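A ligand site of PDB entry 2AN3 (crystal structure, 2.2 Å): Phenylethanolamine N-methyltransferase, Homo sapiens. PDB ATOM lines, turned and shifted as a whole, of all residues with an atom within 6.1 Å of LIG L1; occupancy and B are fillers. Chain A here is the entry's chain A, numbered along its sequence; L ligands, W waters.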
ATOM      1  N   TYR A  35       2.298  12.031 -27.375  1.00  0.00           N
ATOM      2  CA  TYR A  35       2.394  11.234 -26.154  1.00  0.00           C
ATOM      3  C   TYR A  35       2.437  12.184 -24.954  1.00  0.00           C
ATOM      4  O   TYR A  35       1.636  12.066 -24.028  1.00  0.00           O
ATOM      5  CB  TYR A  35       3.659  10.372 -26.165  1.00  0.00           C
ATOM      6  CG  TYR A  35       3.867   9.556 -24.913  1.00  0.00           C
ATOM      7  CD1 TYR A  35       3.174   8.362 -24.710  1.00  0.00           C
ATOM      8  CD2 TYR A  35       4.770   9.963 -23.931  1.00  0.00           C
ATOM      9  CE1 TYR A  35       3.366   7.590 -23.558  1.00  0.00           C
ATOM     10  CE2 TYR A  35       4.970   9.202 -22.777  1.00  0.00           C
ATOM     11  CZ  TYR A  35       4.271   8.020 -22.601  1.00  0.00           C
ATOM     12  OH  TYR A  35       4.488   7.250 -21.477  1.00  0.00           O
ATOM     13  N   ASN A  39      -0.469  12.425 -21.883  1.00  0.00           N
ATOM     14  CA  ASN A  39      -0.246  12.015 -20.506  1.00  0.00           C
ATOM     15  C   ASN A  39       0.422  12.996 -19.565  1.00  0.00           C
ATOM     16  O   ASN A  39       0.442  12.770 -18.360  1.00  0.00           O
ATOM     17  CB  ASN A  39       0.568  10.722 -20.519  1.00  0.00           C
ATOM     18  CG  ASN A  39      -0.094   9.637 -21.349  1.00  0.00           C
ATOM     19  OD1 ASN A  39      -1.155   9.131 -20.992  1.00  0.00           O
ATOM     20  ND2 ASN A  39       0.518   9.298 -22.478  1.00  0.00           N
ATOM     21  N   TYR A  40       0.963  14.086 -20.098  1.00  0.00           N
ATOM     22  CA  TYR A  40       1.625  15.028 -19.217  1.00  0.00           C
ATOM     23  C   TYR A  40       1.224  16.485 -19.396  1.00  0.00           C
ATOM     24  O   TYR A  40       1.938  17.397 -19.011  1.00  0.00           O
ATOM     25  CB  TYR A  40       3.145  14.835 -19.320  1.00  0.00           C
ATOM     26  CG  TYR A  40       3.527  13.428 -18.936  1.00  0.00           C
ATOM     27  CD1 TYR A  40       3.711  12.431 -19.901  1.00  0.00           C
ATOM     28  CD2 TYR A  40       3.607  13.054 -17.586  1.00  0.00           C
ATOM     29  CE1 TYR A  40       3.974  11.105 -19.541  1.00  0.00           C
ATOM     30  CE2 TYR A  40       3.859  11.744 -17.216  1.00  0.00           C
ATOM     31  CZ  TYR A  40       4.037  10.773 -18.190  1.00  0.00           C
ATOM     32  OH  TYR A  40       4.288   9.482 -17.812  1.00  0.00           O
ATOM     33  N   ARG A  44      -4.371  15.268 -16.953  1.00  0.00           N
ATOM     34  CA  ARG A  44      -3.408  14.457 -16.205  1.00  0.00           C
ATOM     35  C   ARG A  44      -2.184  15.283 -15.853  1.00  0.00           C
ATOM     36  O   ARG A  44      -1.517  15.026 -14.837  1.00  0.00           O
ATOM     37  CB  ARG A  44      -2.951  13.259 -17.024  1.00  0.00           C
ATOM     38  CG  ARG A  44      -4.040  12.242 -17.247  1.00  0.00           C
ATOM     39  CD  ARG A  44      -3.559  11.057 -18.045  1.00  0.00           C
ATOM     40  NE  ARG A  44      -4.683  10.178 -18.289  1.00  0.00           N
ATOM     41  CZ  ARG A  44      -4.624   8.987 -18.880  1.00  0.00           C
ATOM     42  NH1 ARG A  44      -3.463   8.500 -19.307  1.00  0.00           N
ATOM     43  NH2 ARG A  44      -5.731   8.287 -19.007  1.00  0.00           N
ATOM     44  N   VAL A  53      -2.967  11.516 -10.938  1.00  0.00           N
ATOM     45  CA  VAL A  53      -1.967  10.492 -11.163  1.00  0.00           C
ATOM     46  C   VAL A  53      -0.545  11.047 -11.112  1.00  0.00           C
ATOM     47  O   VAL A  53       0.379  10.363 -10.680  1.00  0.00           O
ATOM     48  CB  VAL A  53      -2.213   9.750 -12.512  1.00  0.00           C
ATOM     49  CG1 VAL A  53      -2.139  10.730 -13.677  1.00  0.00           C
ATOM     50  CG2 VAL A  53      -1.203   8.608 -12.667  1.00  0.00           C
ATOM     51  N   LYS A  57       2.417   9.714  -8.619  1.00  0.00           N
ATOM     52  CA  LYS A  57       3.678   9.161  -9.056  1.00  0.00           C
ATOM     53  C   LYS A  57       4.859   9.906  -8.403  1.00  0.00           C
ATOM     54  O   LYS A  57       5.757   9.277  -7.852  1.00  0.00           O
ATOM     55  CB  LYS A  57       3.774   9.211 -10.590  1.00  0.00           C
ATOM     56  CG  LYS A  57       2.922   8.139 -11.277  1.00  0.00           C
ATOM     57  CD  LYS A  57       3.068   8.161 -12.791  1.00  0.00           C
ATOM     58  CE  LYS A  57       2.490   9.430 -13.385  1.00  0.00           C
ATOM     59  NZ  LYS A  57       2.605   9.475 -14.881  1.00  0.00           N
ATOM     60  N   PHE A 182       6.304   2.813 -17.247  1.00  0.00           N
ATOM     61  CA  PHE A 182       5.471   2.531 -18.406  1.00  0.00           C
ATOM     62  C   PHE A 182       6.212   1.982 -19.613  1.00  0.00           C
ATOM     63  O   PHE A 182       5.907   2.348 -20.752  1.00  0.00           O
ATOM     64  CB  PHE A 182       4.707   3.798 -18.797  1.00  0.00           C
ATOM     65  CG  PHE A 182       3.895   4.370 -17.674  1.00  0.00           C
ATOM     66  CD1 PHE A 182       4.325   5.508 -16.996  1.00  0.00           C
ATOM     67  CD2 PHE A 182       2.702   3.764 -17.281  1.00  0.00           C
ATOM     68  CE1 PHE A 182       3.580   6.033 -15.932  1.00  0.00           C
ATOM     69  CE2 PHE A 182       1.957   4.280 -16.221  1.00  0.00           C
ATOM     70  CZ  PHE A 182       2.396   5.419 -15.545  1.00  0.00           C
ATOM     71  N   GLU A 185       5.448  -3.334 -19.633  1.00  0.00           N
ATOM     72  CA  GLU A 185       4.109  -3.761 -20.010  1.00  0.00           C
ATOM     73  C   GLU A 185       3.682  -3.173 -21.347  1.00  0.00           C
ATOM     74  O   GLU A 185       2.868  -3.769 -22.064  1.00  0.00           O
ATOM     75  CB  GLU A 185       3.080  -3.397 -18.942  1.00  0.00           C
ATOM     76  CG  GLU A 185       2.675  -1.937 -18.929  1.00  0.00           C
ATOM     77  CD  GLU A 185       3.622  -1.051 -18.156  1.00  0.00           C
ATOM     78  OE1 GLU A 185       4.761  -1.486 -17.863  1.00  0.00           O
ATOM     79  OE2 GLU A 185       3.238   0.093 -17.848  1.00  0.00           O
ATOM     80  N   ALA A 186       4.248  -2.018 -21.702  1.00  0.00           N
ATOM     81  CA  ALA A 186       3.889  -1.356 -22.948  1.00  0.00           C
ATOM     82  C   ALA A 186       4.672  -1.855 -24.166  1.00  0.00           C
ATOM     83  O   ALA A 186       4.476  -1.353 -25.275  1.00  0.00           O
ATOM     84  CB  ALA A 186       4.080   0.154 -22.797  1.00  0.00           C
ATOM     85  N   ALA A 216       1.312   0.625 -15.920  1.00  0.00           N
ATOM     86  CA  ALA A 216      -0.136   0.643 -16.056  1.00  0.00           C
ATOM     87  C   ALA A 216      -0.729  -0.689 -15.601  1.00  0.00           C
ATOM     88  O   ALA A 216      -0.198  -1.765 -15.896  1.00  0.00           O
ATOM     89  CB  ALA A 216      -0.530   0.929 -17.497  1.00  0.00           C
ATOM     90  N   GLU A 219      -4.339  -2.441 -18.387  1.00  0.00           N
ATOM     91  CA  GLU A 219      -4.464  -1.573 -19.548  1.00  0.00           C
ATOM     92  C   GLU A 219      -4.163  -2.439 -20.766  1.00  0.00           C
ATOM     93  O   GLU A 219      -3.415  -3.407 -20.657  1.00  0.00           O
ATOM     94  CB  GLU A 219      -3.467  -0.399 -19.469  1.00  0.00           C
ATOM     95  CG  GLU A 219      -3.222   0.316 -20.801  1.00  0.00           C
ATOM     96  CD  GLU A 219      -2.261   1.504 -20.685  1.00  0.00           C
ATOM     97  OE1 GLU A 219      -2.726   2.674 -20.669  1.00  0.00           O
ATOM     98  OE2 GLU A 219      -1.036   1.265 -20.598  1.00  0.00           O
ATOM     99  N   TRP A 221      -4.173  -0.821 -24.273  1.00  0.00           N
ATOM    100  CA  TRP A 221      -3.771   0.007 -25.397  1.00  0.00           C
ATOM    101  C   TRP A 221      -3.714   1.463 -24.967  1.00  0.00           C
ATOM    102  O   TRP A 221      -4.378   1.856 -24.014  1.00  0.00           O
ATOM    103  CB  TRP A 221      -4.761  -0.109 -26.555  1.00  0.00           C
ATOM    104  CG  TRP A 221      -6.133   0.362 -26.170  1.00  0.00           C
ATOM    105  CD1 TRP A 221      -7.130  -0.393 -25.612  1.00  0.00           C
ATOM    106  CD2 TRP A 221      -6.634   1.699 -26.263  1.00  0.00           C
ATOM    107  NE1 TRP A 221      -8.222   0.391 -25.354  1.00  0.00           N
ATOM    108  CE2 TRP A 221      -7.951   1.685 -25.742  1.00  0.00           C
ATOM    109  CE3 TRP A 221      -6.111   2.915 -26.738  1.00  0.00           C
ATOM    110  CZ2 TRP A 221      -8.745   2.838 -25.682  1.00  0.00           C
ATOM    111  CZ3 TRP A 221      -6.902   4.055 -26.673  1.00  0.00           C
ATOM    112  CH2 TRP A 221      -8.203   4.008 -26.148  1.00  0.00           C
ATOM    113  N   TYR A 222      -2.916   2.250 -25.673  1.00  0.00           N
ATOM    114  CA  TYR A 222      -2.806   3.685 -25.412  1.00  0.00           C
ATOM    115  C   TYR A 222      -2.348   4.296 -26.731  1.00  0.00           C
ATOM    116  O   TYR A 222      -1.673   3.631 -27.513  1.00  0.00           O
ATOM    117  CB  TYR A 222      -1.825   3.974 -24.277  1.00  0.00           C
ATOM    118  CG  TYR A 222      -0.375   3.856 -24.632  1.00  0.00           C
ATOM    119  CD1 TYR A 222       0.339   4.947 -25.119  1.00  0.00           C
ATOM    120  CD2 TYR A 222       0.305   2.645 -24.475  1.00  0.00           C
ATOM    121  CE1 TYR A 222       1.681   4.841 -25.442  1.00  0.00           C
ATOM    122  CE2 TYR A 222       1.650   2.525 -24.792  1.00  0.00           C
ATOM    123  CZ  TYR A 222       2.332   3.634 -25.275  1.00  0.00           C
ATOM    124  OH  TYR A 222       3.650   3.524 -25.615  1.00  0.00           O
ATOM    125  N   VAL A 231      -0.908  -3.146 -25.042  1.00  0.00           N
ATOM    126  CA  VAL A 231      -0.347  -3.243 -23.708  1.00  0.00           C
ATOM    127  C   VAL A 231      -0.796  -4.546 -23.077  1.00  0.00           C
ATOM    128  O   VAL A 231      -1.916  -4.988 -23.292  1.00  0.00           O
ATOM    129  CB  VAL A 231      -0.816  -2.062 -22.803  1.00  0.00           C
ATOM    130  CG1 VAL A 231      -0.165  -2.152 -21.422  1.00  0.00           C
ATOM    131  CG2 VAL A 231      -0.502  -0.736 -23.479  1.00  0.00           C
ATOM    132  N   MET A 258      -7.291   4.817 -11.354  1.00  0.00           N
ATOM    133  CA  MET A 258      -7.524   5.942 -12.243  1.00  0.00           C
ATOM    134  C   MET A 258      -8.923   6.518 -12.075  1.00  0.00           C
ATOM    135  O   MET A 258      -9.921   5.851 -12.361  1.00  0.00           O
ATOM    136  CB  MET A 258      -7.278   5.502 -13.690  1.00  0.00           C
ATOM    137  CG  MET A 258      -6.877   6.654 -14.630  1.00  0.00           C
ATOM    138  SD  MET A 258      -5.307   7.467 -14.204  1.00  0.00           S
ATOM    139  CE  MET A 258      -4.118   6.269 -14.753  1.00  0.00           C
ATOM    140  N   VAL A 266      -7.397   8.393 -24.491  1.00  0.00           N
ATOM    141  CA  VAL A 266      -6.045   8.132 -24.982  1.00  0.00           C
ATOM    142  C   VAL A 266      -5.596   6.721 -24.628  1.00  0.00           C
ATOM    143  O   VAL A 266      -4.546   6.252 -25.086  1.00  0.00           O
ATOM    144  CB  VAL A 266      -5.018   9.141 -24.401  1.00  0.00           C
ATOM    145  CG1 VAL A 266      -5.508  10.555 -24.643  1.00  0.00           C
ATOM    146  CG2 VAL A 266      -4.793   8.885 -22.903  1.00  0.00           C
ATOM    147  N   ASP A 267      -6.398   6.046 -23.806  1.00  0.00           N
ATOM    148  CA  ASP A 267      -6.080   4.689 -23.395  1.00  0.00           C
ATOM    149  C   ASP A 267      -7.242   4.140 -22.583  1.00  0.00           C
ATOM    150  O   ASP A 267      -8.296   4.784 -22.496  1.00  0.00           O
ATOM    151  CB  ASP A 267      -4.808   4.659 -22.538  1.00  0.00           C
ATOM    152  CG  ASP A 267      -4.930   5.501 -21.264  1.00  0.00           C
ATOM    153  OD1 ASP A 267      -5.947   5.378 -20.554  1.00  0.00           O
ATOM    154  OD2 ASP A 267      -3.995   6.267 -20.964  1.00  0.00           O
ATOM    155  N   VAL A 269      -6.430   2.568 -19.419  1.00  0.00           N
ATOM    156  CA  VAL A 269      -5.764   2.208 -18.168  1.00  0.00           C
ATOM    157  C   VAL A 269      -6.767   2.226 -17.009  1.00  0.00           C
ATOM    158  O   VAL A 269      -7.600   3.131 -16.912  1.00  0.00           O
ATOM    159  CB  VAL A 269      -4.601   3.181 -17.860  1.00  0.00           C
ATOM    160  CG1 VAL A 269      -5.136   4.609 -17.693  1.00  0.00           C
ATOM    161  CG2 VAL A 269      -3.878   2.730 -16.596  1.00  0.00           C
ATOM    162  N   GLY A 271      -5.607   1.396 -13.617  1.00  0.00           N
ATOM    163  CA  GLY A 271      -4.862   1.849 -12.463  1.00  0.00           C
ATOM    164  C   GLY A 271      -3.379   1.996 -12.769  1.00  0.00           C
ATOM    165  O   GLY A 271      -2.944   1.751 -13.890  1.00  0.00           O
ATOM    166  N   VAL A 272      -2.607   2.402 -11.776  1.00  0.00           N
ATOM    167  CA  VAL A 272      -1.163   2.557 -11.957  1.00  0.00           C
ATOM    168  C   VAL A 272      -0.461   1.955 -10.752  1.00  0.00           C
ATOM    169  O   VAL A 272      -0.894   2.137  -9.613  1.00  0.00           O
ATOM    170  CB  VAL A 272      -0.766   4.057 -12.077  1.00  0.00           C
ATOM    171  CG1 VAL A 272       0.742   4.194 -12.159  1.00  0.00           C
ATOM    172  CG2 VAL A 272      -1.405   4.676 -13.313  1.00  0.00           C
HETATM  173  C1  LIG L   1      -0.125   4.563 -19.689  1.00  0.00           C
HETATM  174  C2  LIG L   1       1.274   4.490 -20.325  1.00  0.00           C
HETATM  175  C3  LIG L   1       1.679   5.862 -20.871  1.00  0.00           C
HETATM  176  C4  LIG L   1       1.829   6.853 -19.725  1.00  0.00           C
HETATM  177  C5  LIG L   1       0.661   6.804 -18.732  1.00  0.00           C
HETATM  178  C6  LIG L   1       0.511   7.849 -17.822  1.00  0.00           C
HETATM  179  C7  LIG L   1      -0.225   5.728 -18.697  1.00  0.00           C
HETATM  180  C8  LIG L   1      -1.243   5.700 -17.755  1.00  0.00           C
HETATM  181  C9  LIG L   1      -1.391   6.741 -16.837  1.00  0.00           C
HETATM  182  C10 LIG L   1      -0.506   7.821 -16.881  1.00  0.00           C
HETATM  183  O1  LIG L   1      -1.095   4.755 -20.722  1.00  0.00           O
HETATM  184  N1  LIG L   1       1.260   3.499 -21.404  1.00  0.00           N
HETATM  185  N1  LG2 L   2       9.086   6.512 -19.440  1.00  0.00           N
HETATM  186  C1  LG2 L   2       8.111   7.422 -20.019  1.00  0.00           C
HETATM  187  C2  LG2 L   2       7.687   6.918 -21.411  1.00  0.00           C
HETATM  188  C3  LG2 L   2       7.144   5.479 -21.474  1.00  0.00           C
HETATM  189  S1  LG2 L   2       6.376   5.130 -23.091  1.00  0.00           S
HETATM  190  C4  LG2 L   2       6.889   7.692 -19.110  1.00  0.00           C
HETATM  191  O1  LG2 L   2       6.921   7.281 -17.931  1.00  0.00           O
HETATM  192  O2  LG2 L   2       5.927   8.328 -19.564  1.00  0.00           O
HETATM  193  C5  LG2 L   2       7.128   3.525 -23.545  1.00  0.00           C
HETATM  194  C6  LG2 L   2       8.498   3.716 -24.138  1.00  0.00           C
HETATM  195  O3  LG2 L   2       9.183   2.454 -24.362  1.00  0.00           O
HETATM  196  C7  LG2 L   2       8.593   4.499 -25.448  1.00  0.00           C
HETATM  197  O4  LG2 L   2       9.484   5.597 -25.285  1.00  0.00           O
HETATM  198  C8  LG2 L   2       9.074   3.460 -26.451  1.00  0.00           C
HETATM  199  O5  LG2 L   2       9.842   3.961 -27.529  1.00  0.00           O
HETATM  200  C9  LG2 L   2       9.925   2.548 -25.562  1.00  0.00           C
HETATM  201  N2  LG2 L   2      10.158   1.213 -26.103  1.00  0.00           N
HETATM  202  C10 LG2 L   2       9.492   0.549 -27.166  1.00  0.00           C
HETATM  203  N3  LG2 L   2       9.991  -0.626 -27.439  1.00  0.00           N
HETATM  204  C11 LG2 L   2      11.013  -0.764 -26.520  1.00  0.00           C
HETATM  205  C12 LG2 L   2      11.904  -1.843 -26.338  1.00  0.00           C
HETATM  206  N4  LG2 L   2      11.896  -2.943 -27.096  1.00  0.00           N
HETATM  207  N5  LG2 L   2      12.840  -1.730 -25.356  1.00  0.00           N
HETATM  208  C13 LG2 L   2      12.842  -0.595 -24.603  1.00  0.00           C
HETATM  209  N6  LG2 L   2      12.031   0.487 -24.681  1.00  0.00           N
HETATM  210  C14 LG2 L   2      11.130   0.328 -25.680  1.00  0.00           C
HETATM  211  O   HOH W   1       1.830   1.058 -20.192  1.00  0.00           O
HETATM  212  O   HOH W   2      -1.605   6.715 -22.200  1.00  0.00           O
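The side-chain carboxylate (OE2) of Glu 219 is in salt-bridge range of a nitrogen (N1) of LIG L1 (3.3 Å).
An oxygen (O1) of LIG L1 sits at hydrogen-bond distance from the side-chain carboxylate (OD2) of Asp 267 (3.3 Å).
OH of Tyr 35 is in hydrogen-bond range of O2 of LG2 L2.
O2 of LG2 L2 sits at hydrogen-bond distance from OH of Tyr 40, 2.7 Å away.
The backbone carbonyl oxygen of Tyr 35 sits at hydrogen-bond distance from the side-chain amide nitrogen of Asn 39 (3.4 Å).
The guanidinium group (NH1) of Arg 44 is in salt-bridge range of the side-chain carboxylate (OD2) of Asp 267, at 2.8 Å.
N of Val 269 sits at hydrogen-bond distance from OD1 of Asp 267 (3.1 Å).
The guanidinium group of Arg 44 is in hydrogen-bond range of the side-chain amide oxygen of Asn 39 (2.9 Å).
The side-chain amino group of Lys 57 is in hydrogen-bond range of the side-chain hydroxyl of Tyr 40 (3.4 Å).
Merely in contact with LIG L1: Tyr 35, Tyr 222, Phe 182, Met 258, Arg 44, Asn 39 and Lys 57.
Nine residues have an atom within 4 Å of LIG L1: Tyr 35, Asn 39, Arg 44, Lys 57, Phe 182, Glu 219, Tyr 222, Met 258 and Asp 267.
Water W2 lies within hydrogen-bond range of an oxygen (O1) of LIG L1, the side-chain carboxylate (OD2) of Asp 267 and the side-chain amide oxygen (OD1) of Asn 39.
Water W1 lies within hydrogen-bond range of a nitrogen (N1) of LIG L1 (2.8 Å), the side-chain carboxylate (OE2) of Glu 185 (2.9 Å) and the side-chain carboxylate (OE2) of Glu 219 (2.9 Å).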
